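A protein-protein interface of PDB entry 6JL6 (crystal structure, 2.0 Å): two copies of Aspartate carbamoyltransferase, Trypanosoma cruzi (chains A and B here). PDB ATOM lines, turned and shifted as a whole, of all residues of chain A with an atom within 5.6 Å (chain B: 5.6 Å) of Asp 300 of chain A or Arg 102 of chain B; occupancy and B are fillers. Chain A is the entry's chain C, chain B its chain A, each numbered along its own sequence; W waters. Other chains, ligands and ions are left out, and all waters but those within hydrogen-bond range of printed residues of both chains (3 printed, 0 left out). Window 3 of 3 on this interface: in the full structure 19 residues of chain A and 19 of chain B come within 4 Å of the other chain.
The side-chain hydroxyl (OG1) of Thr 96 of chain B sits at hydrogen-bond distance from the backbone NH (N) of Asp 99 of chain B. The backbone carbonyl oxygen (O) of Asp 99 of chain B is in hydrogen-bond range of the side-chain hydroxyl (OG1) of Thr 103 of chain B, at 2.8 Å. The backbone carbonyl oxygen (O) of Thr 103 of chain B is in hydrogen-bond range of the side-chain hydroxyl (OG) of Ser 106 of chain B (2.7 Å). The guanidinium group (NH1) of Arg 291 of chain A sits at hydrogen-bond distance from the backbone carbonyl oxygen (O) of Leu 295 of chain A, at 3.0 Å. The side-chain carboxylate of Asp 300 of chain A is in salt-bridge range of the guanidinium group of Arg 291 of chain A. OD1 of Asp 300 of chain A lies within hydrogen-bond range of OH of Tyr 307 of chain A (2.6 Å).
CD of Arg 102 of chain B touches CZ of Phe 308 of chain A (3.3 Å). CB of Met 311 of chain A touches OG of Ser 106 of chain B (3.8 Å).
OD2 of Asp 99 of chain B lies within salt-bridge range of NE of Arg 291 of chain A. NH1 of Arg 102 of chain B lies within salt-bridge range of OD2 of Asp 300 of chain A, 3.8 Å away. The side-chain sulfur of Met 311 of chain A sits at hydrogen-bond distance from the side-chain hydroxyl of Thr 103 of chain B (3.6 Å).
Of chain B, only Arg 102 (3.8 Å) comes within 4 Å of Asp 300 of chain A. Of the printed residues of chain A, Arg 102 of chain B touches Asp 300 and Phe 308. Of the printed residues of chain B, Phe 308 of chain A touches Arg 102 (3.3 Å). Printed residues of chain A within 4 Å of Thr 103 of chain B: Met 311. Of the printed residues of chain B, Arg 291 of chain A touches Asp 99. Thr 100 of chain B touches none of the printed residues of chain A. The nearest residue of chain B that does not touch Asp 300 of chain A is Asp 99 of chain B (5.0 Å). The nearest printed residue of chain A that does not touch Asp 99 of chain B is Phe 308 of chain A (4.04 Å).
No position is printed for both chains. Of the 5 pairs that touch across the chains among the printed residues, none has its exchanged pair printed and touching as well.
Water W3 lies within hydrogen-bond range of the side-chain carboxylate (OD2) of Asp 300 of chain A (2.6 Å) and the guanidinium group (NH1) of Arg 102 of chain B (2.6 Å). Water W1 lies within hydrogen-bond range of OD2 of Asp 99 of chain B (2.7 Å) and N of Arg 291 of chain A (3.0 Å). Water W2 bridges OG of Ser 106 of chain B (2.9 Å) and O of Met 311 of chain A (2.9 Å).
Printed residues of chain A that touch a printed residue of chain B: Arg 291, Asp 300, Phe 308 and Met 311. Hydrophobic or aromatic side chains of chain A that line the printed part of chain B: Phe 308 and Met 311. Among the printed residues, 5 pairs touch across the chains. Among the printed residues, Asp or Glu carboxylates within 4 Å of a Lys or Arg side-chain nitrogen of the other chain: Arg 291 of chain A with Asp 99 of chain B and Asp 300 of chain A with Arg 102 of chain B.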
ATOM      1  N   ARG A 291      20.013 -13.084   0.882  1.00  0.00           N
ATOM      2  CA  ARG A 291      20.245 -12.369   2.134  1.00  0.00           C
ATOM      3  C   ARG A 291      21.209 -13.138   3.021  1.00  0.00           C
ATOM      4  O   ARG A 291      21.374 -14.351   2.862  1.00  0.00           O
ATOM      5  CB  ARG A 291      18.931 -12.183   2.895  1.00  0.00           C
ATOM      6  CG  ARG A 291      18.272 -13.499   3.310  1.00  0.00           C
ATOM      7  CD  ARG A 291      17.156 -13.356   4.320  1.00  0.00           C
ATOM      8  NE  ARG A 291      16.379 -14.581   4.339  1.00  0.00           N
ATOM      9  CZ  ARG A 291      15.349 -14.815   5.129  1.00  0.00           C
ATOM     10  NH1 ARG A 291      14.962 -13.923   6.053  1.00  0.00           N
ATOM     11  NH2 ARG A 291      14.704 -15.964   5.010  1.00  0.00           N
ATOM     12  N   LEU A 295      18.479  -9.520   7.362  1.00  0.00           N
ATOM     13  CA  LEU A 295      17.050  -9.749   7.368  1.00  0.00           C
ATOM     14  C   LEU A 295      16.764 -11.076   8.030  1.00  0.00           C
ATOM     15  O   LEU A 295      16.955 -12.142   7.443  1.00  0.00           O
ATOM     16  CB  LEU A 295      16.515  -9.717   5.945  1.00  0.00           C
ATOM     17  CG  LEU A 295      15.015  -9.953   5.697  1.00  0.00           C
ATOM     18  CD1 LEU A 295      14.114  -9.062   6.550  1.00  0.00           C
ATOM     19  CD2 LEU A 295      14.717  -9.746   4.220  1.00  0.00           C
ATOM     20  N   SER A 296      16.329 -10.998   9.275  1.00  0.00           N
ATOM     21  CA  SER A 296      16.107 -12.184  10.085  1.00  0.00           C
ATOM     22  C   SER A 296      14.959 -13.063   9.575  1.00  0.00           C
ATOM     23  O   SER A 296      13.894 -12.578   9.161  1.00  0.00           O
ATOM     24  CB  SER A 296      15.834 -11.757  11.530  1.00  0.00           C
ATOM     25  OG  SER A 296      15.460 -12.846  12.341  1.00  0.00           O
ATOM     26  N   THR A 297      15.153 -14.377   9.697  1.00  0.00           N
ATOM     27  CA  THR A 297      14.077 -15.336   9.416  1.00  0.00           C
ATOM     28  C   THR A 297      12.852 -15.139  10.321  1.00  0.00           C
ATOM     29  O   THR A 297      11.774 -15.643   9.999  1.00  0.00           O
ATOM     30  CB  THR A 297      14.561 -16.790   9.567  1.00  0.00           C
ATOM     31  OG1 THR A 297      15.020 -16.988  10.904  1.00  0.00           O
ATOM     32  CG2 THR A 297      15.718 -17.101   8.599  1.00  0.00           C
ATOM     33  N   THR A 298      13.005 -14.406  11.431  1.00  0.00           N
ATOM     34  CA  THR A 298      11.881 -14.114  12.324  1.00  0.00           C
ATOM     35  C   THR A 298      10.829 -13.228  11.667  1.00  0.00           C
ATOM     36  O   THR A 298       9.716 -13.173  12.125  1.00  0.00           O
ATOM     37  CB  THR A 298      12.331 -13.442  13.655  1.00  0.00           C
ATOM     38  OG1 THR A 298      13.043 -12.225  13.385  1.00  0.00           O
ATOM     39  CG2 THR A 298      13.217 -14.371  14.474  1.00  0.00           C
ATOM     40  N   VAL A 299      11.194 -12.540  10.597  1.00  0.00           N
ATOM     41  CA  VAL A 299      10.277 -11.679   9.832  1.00  0.00           C
ATOM     42  C   VAL A 299       9.458 -12.446   8.769  1.00  0.00           C
ATOM     43  O   VAL A 299       8.413 -11.964   8.302  1.00  0.00           O
ATOM     44  CB  VAL A 299      11.101 -10.537   9.185  1.00  0.00           C
ATOM     45  CG1 VAL A 299      10.238  -9.600   8.363  1.00  0.00           C
ATOM     46  CG2 VAL A 299      11.827  -9.771  10.283  1.00  0.00           C
ATOM     47  N   ASP A 300       9.904 -13.648   8.417  1.00  0.00           N
ATOM     48  CA  ASP A 300       9.354 -14.355   7.249  1.00  0.00           C
ATOM     49  C   ASP A 300       7.856 -14.617   7.354  1.00  0.00           C
ATOM     50  O   ASP A 300       7.172 -14.535   6.353  1.00  0.00           O
ATOM     51  CB  ASP A 300      10.093 -15.668   7.013  1.00  0.00           C
ATOM     52  CG  ASP A 300      11.564 -15.463   6.708  1.00  0.00           C
ATOM     53  OD1 ASP A 300      12.014 -14.300   6.530  1.00  0.00           O
ATOM     54  OD2 ASP A 300      12.289 -16.470   6.637  1.00  0.00           O
ATOM     55  N   ALA A 301       7.357 -14.900   8.559  1.00  0.00           N
ATOM     56  CA  ALA A 301       5.919 -15.133   8.789  1.00  0.00           C
ATOM     57  C   ALA A 301       5.058 -13.865   8.704  1.00  0.00           C
ATOM     58  O   ALA A 301       3.832 -13.961   8.571  1.00  0.00           O
ATOM     59  CB  ALA A 301       5.692 -15.807  10.149  1.00  0.00           C
ATOM     60  N   ASP A 302       5.678 -12.688   8.802  1.00  0.00           N
ATOM     61  CA  ASP A 302       4.927 -11.447   8.805  1.00  0.00           C
ATOM     62  C   ASP A 302       4.214 -11.257   7.460  1.00  0.00           C
ATOM     63  O   ASP A 302       4.832 -11.414   6.423  1.00  0.00           O
ATOM     64  CB  ASP A 302       5.861 -10.255   9.098  1.00  0.00           C
ATOM     65  CG  ASP A 302       5.113  -9.020   9.548  1.00  0.00           C
ATOM     66  OD1 ASP A 302       4.218  -8.562   8.827  1.00  0.00           O
ATOM     67  OD2 ASP A 302       5.430  -8.485  10.628  1.00  0.00           O
ATOM     68  N   ALA A 305       6.155  -9.098   5.007  1.00  0.00           N
ATOM     69  CA  ALA A 305       7.348  -9.680   4.384  1.00  0.00           C
ATOM     70  C   ALA A 305       7.030 -10.034   2.916  1.00  0.00           C
ATOM     71  O   ALA A 305       6.365 -11.017   2.638  1.00  0.00           O
ATOM     72  CB  ALA A 305       7.817 -10.914   5.156  1.00  0.00           C
ATOM     73  N   TYR A 307       9.349 -10.303   0.351  1.00  0.00           N
ATOM     74  CA  TYR A 307      10.600 -10.627  -0.390  1.00  0.00           C
ATOM     75  C   TYR A 307      10.579 -11.989  -1.080  1.00  0.00           C
ATOM     76  O   TYR A 307      11.344 -12.233  -2.018  1.00  0.00           O
ATOM     77  CB  TYR A 307      11.872 -10.452   0.481  1.00  0.00           C
ATOM     78  CG  TYR A 307      11.739 -10.847   1.928  1.00  0.00           C
ATOM     79  CD1 TYR A 307      11.250  -9.938   2.881  1.00  0.00           C
ATOM     80  CD2 TYR A 307      12.107 -12.119   2.371  1.00  0.00           C
ATOM     81  CE1 TYR A 307      11.115 -10.295   4.221  1.00  0.00           C
ATOM     82  CE2 TYR A 307      11.991 -12.478   3.715  1.00  0.00           C
ATOM     83  CZ  TYR A 307      11.477 -11.560   4.636  1.00  0.00           C
ATOM     84  OH  TYR A 307      11.348 -11.891   5.991  1.00  0.00           O
ATOM     85  N   PHE A 308       9.716 -12.878  -0.628  1.00  0.00           N
ATOM     86  CA  PHE A 308       9.468 -14.111  -1.374  1.00  0.00           C
ATOM     87  C   PHE A 308       8.485 -13.888  -2.509  1.00  0.00           C
ATOM     88  O   PHE A 308       8.719 -14.357  -3.619  1.00  0.00           O
ATOM     89  CB  PHE A 308       9.008 -15.208  -0.425  1.00  0.00           C
ATOM     90  CG  PHE A 308       9.961 -15.439   0.720  1.00  0.00           C
ATOM     91  CD1 PHE A 308      11.331 -15.522   0.496  1.00  0.00           C
ATOM     92  CD2 PHE A 308       9.489 -15.604   2.012  1.00  0.00           C
ATOM     93  CE1 PHE A 308      12.212 -15.734   1.540  1.00  0.00           C
ATOM     94  CE2 PHE A 308      10.373 -15.842   3.057  1.00  0.00           C
ATOM     95  CZ  PHE A 308      11.738 -15.887   2.814  1.00  0.00           C
ATOM     96  N   MET A 311      10.055 -12.454  -5.680  1.00  0.00           N
ATOM     97  CA  MET A 311      10.664 -13.345  -6.695  1.00  0.00           C
ATOM     98  C   MET A 311       9.641 -13.847  -7.722  1.00  0.00           C
ATOM     99  O   MET A 311       9.968 -13.981  -8.906  1.00  0.00           O
ATOM    100  CB  MET A 311      11.379 -14.523  -6.030  1.00  0.00           C
ATOM    101  CG  MET A 311      12.617 -14.111  -5.253  1.00  0.00           C
ATOM    102  SD  MET A 311      13.586 -15.536  -4.707  1.00  0.00           S
ATOM    103  CE  MET A 311      12.493 -16.081  -3.394  1.00  0.00           C
ATOM    104  N   THR B  96      20.898 -19.705   2.500  1.00  0.00           N
ATOM    105  CA  THR B  96      20.502 -20.931   3.193  1.00  0.00           C
ATOM    106  C   THR B  96      19.774 -21.925   2.271  1.00  0.00           C
ATOM    107  O   THR B  96      19.313 -21.581   1.169  1.00  0.00           O
ATOM    108  CB  THR B  96      19.572 -20.638   4.384  1.00  0.00           C
ATOM    109  OG1 THR B  96      18.412 -19.946   3.924  1.00  0.00           O
ATOM    110  CG2 THR B  96      20.269 -19.795   5.431  1.00  0.00           C
ATOM    111  N   LEU B  97      19.667 -23.154   2.756  1.00  0.00           N
ATOM    112  CA  LEU B  97      18.903 -24.200   2.093  1.00  0.00           C
ATOM    113  C   LEU B  97      17.449 -23.786   1.925  1.00  0.00           C
ATOM    114  O   LEU B  97      16.919 -23.893   0.829  1.00  0.00           O
ATOM    115  CB  LEU B  97      18.959 -25.515   2.887  1.00  0.00           C
ATOM    116  CG  LEU B  97      18.249 -26.698   2.199  1.00  0.00           C
ATOM    117  CD1 LEU B  97      18.805 -26.922   0.798  1.00  0.00           C
ATOM    118  CD2 LEU B  97      18.352 -27.963   3.037  1.00  0.00           C
ATOM    119  N   ALA B  98      16.826 -23.297   2.996  1.00  0.00           N
ATOM    120  CA  ALA B  98      15.429 -22.879   2.948  1.00  0.00           C
ATOM    121  C   ALA B  98      15.171 -21.769   1.902  1.00  0.00           C
ATOM    122  O   ALA B  98      14.205 -21.850   1.142  1.00  0.00           O
ATOM    123  CB  ALA B  98      14.954 -22.431   4.318  1.00  0.00           C
ATOM    124  N   ASP B  99      16.049 -20.766   1.861  1.00  0.00           N
ATOM    125  CA  ASP B  99      15.927 -19.667   0.892  1.00  0.00           C
ATOM    126  C   ASP B  99      16.120 -20.143  -0.564  1.00  0.00           C
ATOM    127  O   ASP B  99      15.429 -19.666  -1.449  1.00  0.00           O
ATOM    128  CB  ASP B  99      16.900 -18.535   1.217  1.00  0.00           C
ATOM    129  CG  ASP B  99      16.434 -17.644   2.393  1.00  0.00           C
ATOM    130  OD1 ASP B  99      15.343 -17.847   2.967  1.00  0.00           O
ATOM    131  OD2 ASP B  99      17.181 -16.700   2.738  1.00  0.00           O
ATOM    132  N   THR B 100      17.074 -21.056  -0.794  1.00  0.00           N
ATOM    133  CA  THR B 100      17.271 -21.710  -2.099  1.00  0.00           C
ATOM    134  C   THR B 100      15.996 -22.421  -2.533  1.00  0.00           C
ATOM    135  O   THR B 100      15.566 -22.275  -3.677  1.00  0.00           O
ATOM    136  CB  THR B 100      18.439 -22.718  -2.082  1.00  0.00           C
ATOM    137  OG1 THR B 100      19.625 -22.047  -1.654  1.00  0.00           O
ATOM    138  CG2 THR B 100      18.677 -23.310  -3.492  1.00  0.00           C
ATOM    139  N   ILE B 101      15.366 -23.132  -1.604  1.00  0.00           N
ATOM    140  CA  ILE B 101      14.113 -23.813  -1.872  1.00  0.00           C
ATOM    141  C   ILE B 101      13.012 -22.824  -2.229  1.00  0.00           C
ATOM    142  O   ILE B 101      12.285 -23.038  -3.202  1.00  0.00           O
ATOM    143  CB  ILE B 101      13.629 -24.681  -0.687  1.00  0.00           C
ATOM    144  CG1 ILE B 101      14.566 -25.873  -0.471  1.00  0.00           C
ATOM    145  CG2 ILE B 101      12.222 -25.203  -0.941  1.00  0.00           C
ATOM    146  CD1 ILE B 101      14.447 -26.971  -1.513  1.00  0.00           C
ATOM    147  N   ARG B 102      12.868 -21.772  -1.433  1.00  0.00           N
ATOM    148  CA  ARG B 102      11.886 -20.725  -1.749  1.00  0.00           C
ATOM    149  C   ARG B 102      12.113 -20.091  -3.139  1.00  0.00           C
ATOM    150  O   ARG B 102      11.151 -19.828  -3.852  1.00  0.00           O
ATOM    151  CB  ARG B 102      11.878 -19.644  -0.680  1.00  0.00           C
ATOM    152  CG  ARG B 102      11.328 -20.117   0.649  1.00  0.00           C
ATOM    153  CD  ARG B 102      11.374 -18.954   1.607  1.00  0.00           C
ATOM    154  NE  ARG B 102      10.865 -19.280   2.932  1.00  0.00           N
ATOM    155  CZ  ARG B 102      11.610 -19.512   4.014  1.00  0.00           C
ATOM    156  NH1 ARG B 102      10.984 -19.774   5.169  1.00  0.00           N
ATOM    157  NH2 ARG B 102      12.960 -19.495   3.974  1.00  0.00           N
ATOM    158  N   THR B 103      13.375 -19.870  -3.500  1.00  0.00           N
ATOM    159  CA  THR B 103      13.745 -19.336  -4.807  1.00  0.00           C
ATOM    160  C   THR B 103      13.252 -20.234  -5.961  1.00  0.00           C
ATOM    161  O   THR B 103      12.508 -19.785  -6.858  1.00  0.00           O
ATOM    162  CB  THR B 103      15.274 -19.116  -4.908  1.00  0.00           C
ATOM    163  OG1 THR B 103      15.709 -18.283  -3.824  1.00  0.00           O
ATOM    164  CG2 THR B 103      15.661 -18.471  -6.222  1.00  0.00           C
ATOM    165  N   LEU B 104      13.639 -21.500  -5.917  1.00  0.00           N
ATOM    166  CA  LEU B 104      13.225 -22.471  -6.951  1.00  0.00           C
ATOM    167  C   LEU B 104      11.688 -22.623  -6.981  1.00  0.00           C
ATOM    168  O   LEU B 104      11.073 -22.682  -8.051  1.00  0.00           O
ATOM    169  CB  LEU B 104      13.932 -23.824  -6.753  1.00  0.00           C
ATOM    170  CG  LEU B 104      15.412 -23.926  -7.166  1.00  0.00           C
ATOM    171  CD1 LEU B 104      15.579 -23.430  -8.569  1.00  0.00           C
ATOM    172  CD2 LEU B 104      16.426 -23.155  -6.332  1.00  0.00           C
ATOM    173  N   ASP B 105      11.092 -22.599  -5.792  1.00  0.00           N
ATOM    174  CA  ASP B 105       9.642 -22.648  -5.597  1.00  0.00           C
ATOM    175  C   ASP B 105       8.861 -21.487  -6.237  1.00  0.00           C
ATOM    176  O   ASP B 105       7.696 -21.643  -6.566  1.00  0.00           O
ATOM    177  CB  ASP B 105       9.351 -22.654  -4.095  1.00  0.00           C
ATOM    178  CG  ASP B 105       8.222 -23.555  -3.703  1.00  0.00           C
ATOM    179  OD1 ASP B 105       7.936 -24.570  -4.367  1.00  0.00           O
ATOM    180  OD2 ASP B 105       7.646 -23.270  -2.648  1.00  0.00           O
ATOM    181  N   SER B 106       9.490 -20.326  -6.384  1.00  0.00           N
ATOM    182  CA  SER B 106       8.830 -19.159  -6.970  1.00  0.00           C
ATOM    183  C   SER B 106       8.522 -19.312  -8.470  1.00  0.00           C
ATOM    184  O   SER B 106       7.652 -18.602  -8.981  1.00  0.00           O
ATOM    185  CB  SER B 106       9.672 -17.904  -6.766  1.00  0.00           C
ATOM    186  OG  SER B 106      10.778 -17.873  -7.662  1.00  0.00           O
ATOM    187  N   VAL B 127       9.233 -25.547   3.971  1.00  0.00           N
ATOM    188  CA  VAL B 127       9.104 -24.268   3.264  1.00  0.00           C
ATOM    189  C   VAL B 127       8.546 -24.374   1.829  1.00  0.00           C
ATOM    190  O   VAL B 127       7.993 -23.407   1.334  1.00  0.00           O
ATOM    191  CB  VAL B 127      10.437 -23.472   3.252  1.00  0.00           C
ATOM    192  CG1 VAL B 127      10.916 -23.195   4.677  1.00  0.00           C
ATOM    193  CG2 VAL B 127      11.519 -24.185   2.459  1.00  0.00           C
HETATM  194  O   HOH W   1      18.503 -15.616   0.621  1.00  0.00           O
HETATM  195  O   HOH W   2      11.384 -16.288  -9.982  1.00  0.00           O
HETATM  196  O   HOH W   3      11.840 -18.870   7.501  1.00  0.00           O
